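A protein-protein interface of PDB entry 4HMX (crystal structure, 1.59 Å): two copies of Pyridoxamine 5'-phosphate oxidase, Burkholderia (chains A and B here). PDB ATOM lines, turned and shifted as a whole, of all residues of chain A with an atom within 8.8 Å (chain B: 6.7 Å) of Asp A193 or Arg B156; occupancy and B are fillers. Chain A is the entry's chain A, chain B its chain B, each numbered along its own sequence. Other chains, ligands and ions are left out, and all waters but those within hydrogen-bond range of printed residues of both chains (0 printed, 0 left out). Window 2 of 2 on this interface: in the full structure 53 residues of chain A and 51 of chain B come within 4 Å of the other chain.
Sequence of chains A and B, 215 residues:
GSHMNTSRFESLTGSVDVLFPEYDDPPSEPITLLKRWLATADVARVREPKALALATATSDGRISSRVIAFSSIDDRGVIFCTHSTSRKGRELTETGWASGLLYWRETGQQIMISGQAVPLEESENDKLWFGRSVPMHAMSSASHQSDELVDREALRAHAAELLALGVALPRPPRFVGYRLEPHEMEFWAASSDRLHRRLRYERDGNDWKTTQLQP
Among the printed residues, pairs that only touch across the chains: Ser A191 with Arg B152 (3.7 Å), Asp A193 with Met B139 (3.6 Å), Arg A194 with Pro B135 (3.6 Å), Arg A194 with Met B139 (3.9 Å), Leu A195 with Arg B156 (3.8 Å), His A196 with Arg B152 (3.6 Å) and Arg A197 with Arg B152 (3.8 Å).
No position is printed for both chains.
The side-chain hydroxyl (OH) of Tyr A23 sits at hydrogen-bond distance from the guanidinium group (NH2) of Arg B152 (3.3 Å).
The side-chain carboxylate of Asp A193 is in salt-bridge range of the guanidinium group of Arg B156, at 2.6 Å.
The backbone carbonyl oxygen (O) of Leu A195 sits at hydrogen-bond distance from the guanidinium group (NH1) of Arg B152.
The backbone NH (N) of Ala A189 sits at hydrogen-bond distance from the backbone carbonyl oxygen (O) of Arg A197, 2.9 Å away.
The side-chain hydroxyl (OG) of Ser A191 sits at hydrogen-bond distance from the backbone carbonyl oxygen (O) of Leu A195.
A ring nitrogen (ND1) of His A196 lies within hydrogen-bond range of the backbone NH of Ser A191 (3.1 Å).
The side-chain hydroxyl (OG) of Ser A191 is in hydrogen-bond range of the guanidinium group (NE) of Arg A197 (2.9 Å).
OD1 of Asp A193 lies within hydrogen-bond range of N of Leu A195, at 3.0 Å.
The side-chain carboxylate of Glu B153 is in salt-bridge range of the guanidinium group of Arg B156.
Asp A193 touches just these residues of chain B: Met B139 (3.6 Å) and Arg B156 (2.6 Å).
Of chain A, only Asp A193 and Leu A195 come within 4 Å of Arg B156.
No residue of chain A comes within 4 Å of Ala B157.
Of the printed residues of chain B, Tyr A23 touches Arg B152.
Of the printed residues of chain B, Arg A194 touches Pro B135 and Met B139.
Printed residues of chain B within 4 Å of His A196: Arg B152 (3.6 Å).
Ala B159 touches none of the printed residues of chain A.
The nearest printed residue of chain B that does not touch His A196 is Met B139 (6.5 Å).
Of the 13 printed residues of chain A, 7 touch a printed residue of chain B.
Printed residues of chain A that touch a printed residue of chain B: Tyr A23, Ser A191, Asp A193, Arg A194, Leu A195, His A196 and Arg A197.
Hydrophobic or aromatic side chains of chain A within 4 Å of the printed part of chain B: Tyr A23 and Leu A195.
Hydrophobic or aromatic side chains of chain B that line the printed part of chain A: Pro B135 and Met B139.
Among the printed residues, 10 pairs touch across the chains.
Among the printed residues, Asp or Glu carboxylates within 4 Å of a Lys or Arg side-chain nitrogen of the other chain: Asp A193 with Arg B156 (2.6 Å).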
ATOM      1  N   VAL A  16     -16.567  35.410 -24.708  1.00  0.00           N
ATOM      2  CA  VAL A  16     -16.902  34.915 -23.369  1.00  0.00           C
ATOM      3  C   VAL A  16     -17.155  36.060 -22.381  1.00  0.00           C
ATOM      4  O   VAL A  16     -16.652  37.165 -22.542  1.00  0.00           O
ATOM      5  CB  VAL A  16     -15.784  34.036 -22.780  1.00  0.00           C
ATOM      6  CG1 VAL A  16     -15.892  34.013 -21.311  1.00  0.00           C
ATOM      7  CG2 VAL A  16     -15.837  32.626 -23.321  1.00  0.00           C
ATOM      8  N   ASP A  17     -17.948  35.785 -21.354  1.00  0.00           N
ATOM      9  CA  ASP A  17     -18.209  36.747 -20.307  1.00  0.00           C
ATOM     10  C   ASP A  17     -18.867  38.032 -20.802  1.00  0.00           C
ATOM     11  O   ASP A  17     -18.690  39.103 -20.176  1.00  0.00           O
ATOM     12  CB  ASP A  17     -16.898  37.077 -19.548  1.00  0.00           C
ATOM     13  CG  ASP A  17     -16.261  35.839 -18.885  1.00  0.00           C
ATOM     14  OD1 ASP A  17     -16.988  34.917 -18.456  1.00  0.00           O
ATOM     15  OD2 ASP A  17     -15.007  35.774 -18.822  1.00  0.00           O
ATOM     16  N   TYR A  23     -29.398  38.505 -16.151  1.00  0.00           N
ATOM     17  CA  TYR A  23     -29.338  37.166 -15.590  1.00  0.00           C
ATOM     18  C   TYR A  23     -29.872  37.169 -14.150  1.00  0.00           C
ATOM     19  O   TYR A  23     -30.607  36.282 -13.756  1.00  0.00           O
ATOM     20  CB  TYR A  23     -27.908  36.708 -15.647  1.00  0.00           C
ATOM     21  CG  TYR A  23     -27.565  35.378 -15.006  1.00  0.00           C
ATOM     22  CD1 TYR A  23     -28.087  34.183 -15.489  1.00  0.00           C
ATOM     23  CD2 TYR A  23     -26.636  35.321 -14.003  1.00  0.00           C
ATOM     24  CE1 TYR A  23     -27.711  32.962 -14.932  1.00  0.00           C
ATOM     25  CE2 TYR A  23     -26.276  34.137 -13.435  1.00  0.00           C
ATOM     26  CZ  TYR A  23     -26.792  32.963 -13.922  1.00  0.00           C
ATOM     27  OH  TYR A  23     -26.349  31.803 -13.351  1.00  0.00           O
ATOM     28  N   ALA A 189     -25.226  32.447 -22.047  1.00  0.00           N
ATOM     29  CA  ALA A 189     -24.038  33.248 -22.312  1.00  0.00           C
ATOM     30  C   ALA A 189     -22.812  32.560 -21.703  1.00  0.00           C
ATOM     31  O   ALA A 189     -22.770  32.284 -20.495  1.00  0.00           O
ATOM     32  CB  ALA A 189     -24.185  34.668 -21.723  1.00  0.00           C
ATOM     33  N   ALA A 190     -21.812  32.322 -22.544  1.00  0.00           N
ATOM     34  CA  ALA A 190     -20.624  31.565 -22.149  1.00  0.00           C
ATOM     35  C   ALA A 190     -19.862  32.333 -21.086  1.00  0.00           C
ATOM     36  O   ALA A 190     -19.799  33.541 -21.131  1.00  0.00           O
ATOM     37  CB  ALA A 190     -19.710  31.315 -23.351  1.00  0.00           C
ATOM     38  N   SER A 191     -19.226  31.583 -20.195  1.00  0.00           N
ATOM     39  CA  SER A 191     -18.412  32.102 -19.097  1.00  0.00           C
ATOM     40  C   SER A 191     -17.059  31.448 -19.178  1.00  0.00           C
ATOM     41  O   SER A 191     -16.967  30.242 -19.403  1.00  0.00           O
ATOM     42  CB  SER A 191     -19.048  31.764 -17.758  1.00  0.00           C
ATOM     43  OG  SER A 191     -20.154  32.589 -17.565  1.00  0.00           O
ATOM     44  N   SER A 192     -15.994  32.232 -18.999  1.00  0.00           N
ATOM     45  CA  SER A 192     -14.641  31.687 -19.088  1.00  0.00           C
ATOM     46  C   SER A 192     -14.329  30.661 -18.002  1.00  0.00           C
ATOM     47  O   SER A 192     -13.389  29.870 -18.155  1.00  0.00           O
ATOM     48  CB  SER A 192     -13.620  32.821 -19.054  1.00  0.00           C
ATOM     49  OG  SER A 192     -13.774  33.616 -17.883  1.00  0.00           O
ATOM     50  N   ASP A 193     -15.076  30.687 -16.904  1.00  0.00           N
ATOM     51  CA  ASP A 193     -14.900  29.717 -15.793  1.00  0.00           C
ATOM     52  C   ASP A 193     -15.810  28.488 -15.934  1.00  0.00           C
ATOM     53  O   ASP A 193     -15.914  27.652 -15.014  1.00  0.00           O
ATOM     54  CB  ASP A 193     -15.098  30.410 -14.437  1.00  0.00           C
ATOM     55  CG  ASP A 193     -16.537  30.762 -14.145  1.00  0.00           C
ATOM     56  OD1 ASP A 193     -17.417  30.603 -14.999  1.00  0.00           O
ATOM     57  OD2 ASP A 193     -16.780  31.234 -13.003  1.00  0.00           O
ATOM     58  N   ARG A 194     -16.452  28.404 -17.096  1.00  0.00           N
ATOM     59  CA  ARG A 194     -17.337  27.280 -17.461  1.00  0.00           C
ATOM     60  C   ARG A 194     -18.684  27.256 -16.757  1.00  0.00           C
ATOM     61  O   ARG A 194     -19.498  26.371 -17.054  1.00  0.00           O
ATOM     62  CB  ARG A 194     -16.665  25.931 -17.215  1.00  0.00           C
ATOM     63  CG  ARG A 194     -15.491  25.653 -18.113  1.00  0.00           C
ATOM     64  CD  ARG A 194     -15.028  24.211 -17.861  1.00  0.00           C
ATOM     65  NE  ARG A 194     -14.552  23.623 -19.105  1.00  0.00           N
ATOM     66  CZ  ARG A 194     -13.283  23.646 -19.491  1.00  0.00           C
ATOM     67  NH1 ARG A 194     -12.353  24.211 -18.707  1.00  0.00           N
ATOM     68  NH2 ARG A 194     -12.945  23.095 -20.658  1.00  0.00           N
ATOM     69  N   LEU A 195     -18.922  28.174 -15.824  1.00  0.00           N
ATOM     70  CA  LEU A 195     -20.242  28.279 -15.192  1.00  0.00           C
ATOM     71  C   LEU A 195     -21.095  29.260 -16.029  1.00  0.00           C
ATOM     72  O   LEU A 195     -21.363  30.414 -15.664  1.00  0.00           O
ATOM     73  CB  LEU A 195     -20.112  28.687 -13.745  1.00  0.00           C
ATOM     74  CG  LEU A 195     -21.159  28.106 -12.751  1.00  0.00           C
ATOM     75  CD1 LEU A 195     -20.837  28.440 -11.307  1.00  0.00           C
ATOM     76  CD2 LEU A 195     -22.550  28.628 -13.113  1.00  0.00           C
ATOM     77  N   HIS A 196     -21.494  28.751 -17.184  1.00  0.00           N
ATOM     78  CA  HIS A 196     -22.263  29.527 -18.141  1.00  0.00           C
ATOM     79  C   HIS A 196     -23.527  30.068 -17.518  1.00  0.00           C
ATOM     80  O   HIS A 196     -24.093  29.447 -16.638  1.00  0.00           O
ATOM     81  CB  HIS A 196     -22.593  28.640 -19.362  1.00  0.00           C
ATOM     82  CG  HIS A 196     -21.392  27.955 -19.907  1.00  0.00           C
ATOM     83  ND1 HIS A 196     -20.278  28.678 -20.249  1.00  0.00           N
ATOM     84  CD2 HIS A 196     -21.100  26.654 -20.155  1.00  0.00           C
ATOM     85  CE1 HIS A 196     -19.345  27.862 -20.708  1.00  0.00           C
ATOM     86  NE2 HIS A 196     -19.817  26.626 -20.657  1.00  0.00           N
ATOM     87  N   ARG A 197     -23.950  31.244 -17.967  1.00  0.00           N
ATOM     88  CA  ARG A 197     -25.128  31.917 -17.443  1.00  0.00           C
ATOM     89  C   ARG A 197     -26.313  31.468 -18.300  1.00  0.00           C
ATOM     90  O   ARG A 197     -26.333  31.669 -19.526  1.00  0.00           O
ATOM     91  CB  ARG A 197     -24.960  33.453 -17.527  1.00  0.00           C
ATOM     92  CG  ARG A 197     -23.978  34.156 -16.567  1.00  0.00           C
ATOM     93  CD  ARG A 197     -22.557  34.132 -17.009  1.00  0.00           C
ATOM     94  NE  ARG A 197     -22.145  34.515 -18.391  1.00  0.00           N
ATOM     95  CZ  ARG A 197     -21.929  35.769 -18.835  1.00  0.00           C
ATOM     96  NH1 ARG A 197     -22.163  36.831 -18.082  1.00  0.00           N
ATOM     97  NH2 ARG A 197     -21.502  35.969 -20.056  1.00  0.00           N
ATOM     98  N   PRO A 215     -25.083  24.682 -15.664  1.00  0.00           N
ATOM     99  CA  PRO A 215     -24.536  24.600 -17.032  1.00  0.00           C
ATOM    100  C   PRO A 215     -24.263  23.190 -17.480  1.00  0.00           C
ATOM    101  O   PRO A 215     -24.067  22.255 -16.659  1.00  0.00           O
ATOM    102  CB  PRO A 215     -23.231  25.387 -16.958  1.00  0.00           C
ATOM    103  CG  PRO A 215     -22.806  25.290 -15.457  1.00  0.00           C
ATOM    104  CD  PRO A 215     -24.168  25.335 -14.716  1.00  0.00           C
ATOM    105  OXT PRO A 215     -24.178  22.995 -18.712  1.00  0.00           O
ATOM    106  N   PRO B 135     -10.239  20.473 -15.363  1.00  0.00           N
ATOM    107  CA  PRO B 135     -11.258  21.526 -15.124  1.00  0.00           C
ATOM    108  C   PRO B 135     -12.630  21.202 -15.715  1.00  0.00           C
ATOM    109  O   PRO B 135     -13.656  21.528 -15.097  1.00  0.00           O
ATOM    110  CB  PRO B 135     -10.669  22.771 -15.818  1.00  0.00           C
ATOM    111  CG  PRO B 135      -9.223  22.518 -15.882  1.00  0.00           C
ATOM    112  CD  PRO B 135      -8.996  21.012 -15.939  1.00  0.00           C
ATOM    113  N   MET B 139     -16.128  20.883 -13.358  1.00  0.00           N
ATOM    114  CA  MET B 139     -17.409  21.560 -13.523  1.00  0.00           C
ATOM    115  C   MET B 139     -18.521  20.583 -13.919  1.00  0.00           C
ATOM    116  O   MET B 139     -19.666  20.683 -13.433  1.00  0.00           O
ATOM    117  CB  MET B 139     -17.307  22.716 -14.510  1.00  0.00           C
ATOM    118  CG  MET B 139     -18.613  23.516 -14.617  1.00  0.00           C
ATOM    119  SD  MET B 139     -19.153  24.332 -13.080  1.00  0.00           S
ATOM    120  CE  MET B 139     -17.800  25.502 -12.846  1.00  0.00           C
ATOM    121  N   ALA B 142     -19.551  18.903 -10.729  1.00  0.00           N
ATOM    122  CA  ALA B 142     -20.260  19.836  -9.821  1.00  0.00           C
ATOM    123  C   ALA B 142     -21.664  20.231 -10.281  1.00  0.00           C
ATOM    124  O   ALA B 142     -22.537  20.560  -9.457  1.00  0.00           O
ATOM    125  CB  ALA B 142     -19.438  21.098  -9.589  1.00  0.00           C
ATOM    126  N   ASP B 151     -27.507  28.135  -6.061  1.00  0.00           N
ATOM    127  CA  ASP B 151     -26.430  28.877  -5.463  1.00  0.00           C
ATOM    128  C   ASP B 151     -25.192  28.803  -6.355  1.00  0.00           C
ATOM    129  O   ASP B 151     -24.420  27.832  -6.284  1.00  0.00           O
ATOM    130  CB  ASP B 151     -26.111  28.274  -4.099  1.00  0.00           C
ATOM    131  CG  ASP B 151     -25.153  29.124  -3.289  1.00  0.00           C
ATOM    132  OD1 ASP B 151     -24.366  29.916  -3.862  1.00  0.00           O
ATOM    133  OD2 ASP B 151     -25.191  28.986  -2.051  1.00  0.00           O
ATOM    134  N   ARG B 152     -25.005  29.847  -7.164  1.00  0.00           N
ATOM    135  CA  ARG B 152     -23.927  29.913  -8.142  1.00  0.00           C
ATOM    136  C   ARG B 152     -22.558  29.875  -7.478  1.00  0.00           C
ATOM    137  O   ARG B 152     -21.655  29.115  -7.896  1.00  0.00           O
ATOM    138  CB  ARG B 152     -24.096  31.155  -9.036  1.00  0.00           C
ATOM    139  CG  ARG B 152     -23.026  31.335 -10.097  1.00  0.00           C
ATOM    140  CD  ARG B 152     -23.362  32.478 -11.118  1.00  0.00           C
ATOM    141  NE  ARG B 152     -22.207  32.669 -12.008  1.00  0.00           N
ATOM    142  CZ  ARG B 152     -22.077  32.240 -13.268  1.00  0.00           C
ATOM    143  NH1 ARG B 152     -20.926  32.471 -13.939  1.00  0.00           N
ATOM    144  NH2 ARG B 152     -23.092  31.633 -13.905  1.00  0.00           N
ATOM    145  N   GLU B 153     -22.387  30.641  -6.418  1.00  0.00           N
ATOM    146  CA  GLU B 153     -21.085  30.656  -5.781  1.00  0.00           C
ATOM    147  C   GLU B 153     -20.739  29.307  -5.147  1.00  0.00           C
ATOM    148  O   GLU B 153     -19.588  28.919  -5.160  1.00  0.00           O
ATOM    149  CB  GLU B 153     -20.976  31.796  -4.765  1.00  0.00           C
ATOM    150  CG  GLU B 153     -20.997  33.170  -5.436  1.00  0.00           C
ATOM    151  CD  GLU B 153     -20.073  33.252  -6.659  1.00  0.00           C
ATOM    152  OE1 GLU B 153     -18.848  32.952  -6.523  1.00  0.00           O
ATOM    153  OE2 GLU B 153     -20.575  33.613  -7.757  1.00  0.00           O
ATOM    154  N   ALA B 154     -21.725  28.596  -4.603  1.00  0.00           N
ATOM    155  CA  ALA B 154     -21.469  27.270  -4.023  1.00  0.00           C
ATOM    156  C   ALA B 154     -21.035  26.295  -5.103  1.00  0.00           C
ATOM    157  O   ALA B 154     -20.111  25.498  -4.903  1.00  0.00           O
ATOM    158  CB  ALA B 154     -22.700  26.740  -3.317  1.00  0.00           C
ATOM    159  N   LEU B 155     -21.716  26.356  -6.255  1.00  0.00           N
ATOM    160  CA  LEU B 155     -21.331  25.511  -7.371  1.00  0.00           C
ATOM    161  C   LEU B 155     -19.885  25.804  -7.803  1.00  0.00           C
ATOM    162  O   LEU B 155     -19.056  24.894  -7.972  1.00  0.00           O
ATOM    163  CB  LEU B 155     -22.306  25.677  -8.535  1.00  0.00           C
ATOM    164  CG  LEU B 155     -22.413  24.509  -9.547  1.00  0.00           C
ATOM    165  CD1 LEU B 155     -23.412  24.882 -10.581  1.00  0.00           C
ATOM    166  CD2 LEU B 155     -21.173  24.236 -10.227  1.00  0.00           C
ATOM    167  N   ARG B 156     -19.566  27.068  -8.008  1.00  0.00           N
ATOM    168  CA  ARG B 156     -18.212  27.424  -8.386  1.00  0.00           C
ATOM    169  C   ARG B 156     -17.178  26.915  -7.369  1.00  0.00           C
ATOM    170  O   ARG B 156     -16.136  26.386  -7.749  1.00  0.00           O
ATOM    171  CB  ARG B 156     -18.110  28.935  -8.526  1.00  0.00           C
ATOM    172  CG  ARG B 156     -16.851  29.396  -9.218  1.00  0.00           C
ATOM    173  CD  ARG B 156     -16.867  30.917  -9.312  1.00  0.00           C
ATOM    174  NE  ARG B 156     -17.577  31.355 -10.511  1.00  0.00           N
ATOM    175  CZ  ARG B 156     -18.537  32.288 -10.569  1.00  0.00           C
ATOM    176  NH1 ARG B 156     -18.961  32.926  -9.483  1.00  0.00           N
ATOM    177  NH2 ARG B 156     -19.079  32.590 -11.739  1.00  0.00           N
ATOM    178  N   ALA B 157     -17.488  27.080  -6.076  1.00  0.00           N
ATOM    179  CA  ALA B 157     -16.600  26.645  -4.979  1.00  0.00           C
ATOM    180  C   ALA B 157     -16.410  25.126  -4.970  1.00  0.00           C
ATOM    181  O   ALA B 157     -15.301  24.621  -4.715  1.00  0.00           O
ATOM    182  CB  ALA B 157     -17.170  27.107  -3.593  1.00  0.00           C
ATOM    183  N   HIS B 158     -17.474  24.382  -5.240  1.00  0.00           N
ATOM    184  CA  HIS B 158     -17.322  22.915  -5.285  1.00  0.00           C
ATOM    185  C   HIS B 158     -16.447  22.502  -6.477  1.00  0.00           C
ATOM    186  O   HIS B 158     -15.639  21.614  -6.363  1.00  0.00           O
ATOM    187  CB  HIS B 158     -18.681  22.167  -5.322  1.00  0.00           C
ATOM    188  CG  HIS B 158     -19.466  22.291  -4.071  1.00  0.00           C
ATOM    189  ND1 HIS B 158     -18.912  22.063  -2.827  1.00  0.00           N
ATOM    190  CD2 HIS B 158     -20.763  22.648  -3.852  1.00  0.00           C
ATOM    191  CE1 HIS B 158     -19.837  22.237  -1.901  1.00  0.00           C
ATOM    192  NE2 HIS B 158     -20.968  22.584  -2.492  1.00  0.00           N
ATOM    193  N   ALA B 159     -16.654  23.100  -7.664  1.00  0.00           N
ATOM    194  CA  ALA B 159     -15.802  22.744  -8.799  1.00  0.00           C
ATOM    195  C   ALA B 159     -14.345  23.043  -8.461  1.00  0.00           C
ATOM    196  O   ALA B 159     -13.466  22.227  -8.748  1.00  0.00           O
ATOM    197  CB  ALA B 159     -16.257  23.429 -10.085  1.00  0.00           C
ATOM    198  N   ALA B 160     -14.074  24.153  -7.783  1.00  0.00           N
ATOM    199  CA  ALA B 160     -12.702  24.433  -7.354  1.00  0.00           C
ATOM    200  C   ALA B 160     -12.143  23.396  -6.344  1.00  0.00           C
ATOM    201  O   ALA B 160     -10.973  22.993  -6.413  1.00  0.00           O
ATOM    202  CB  ALA B 160     -12.611  25.835  -6.777  1.00  0.00           C
ATOM    203  N   GLU B 161     -12.966  22.995  -5.385  1.00  0.00           N
ATOM    204  CA  GLU B 161     -12.574  21.936  -4.444  1.00  0.00           C
ATOM    205  C   GLU B 161     -12.142  20.658  -5.170  1.00  0.00           C
ATOM    206  O   GLU B 161     -11.098  20.069  -4.833  1.00  0.00           O
ATOM    207  CB  GLU B 161     -13.742  21.580  -3.514  1.00  0.00           C
ATOM    208  CG  GLU B 161     -13.978  22.573  -2.381  1.00  0.00           C
ATOM    209  CD  GLU B 161     -15.362  22.406  -1.758  1.00  0.00           C
ATOM    210  OE1 GLU B 161     -16.181  21.576  -2.271  1.00  0.00           O
ATOM    211  OE2 GLU B 161     -15.615  23.110  -0.750  1.00  0.00           O
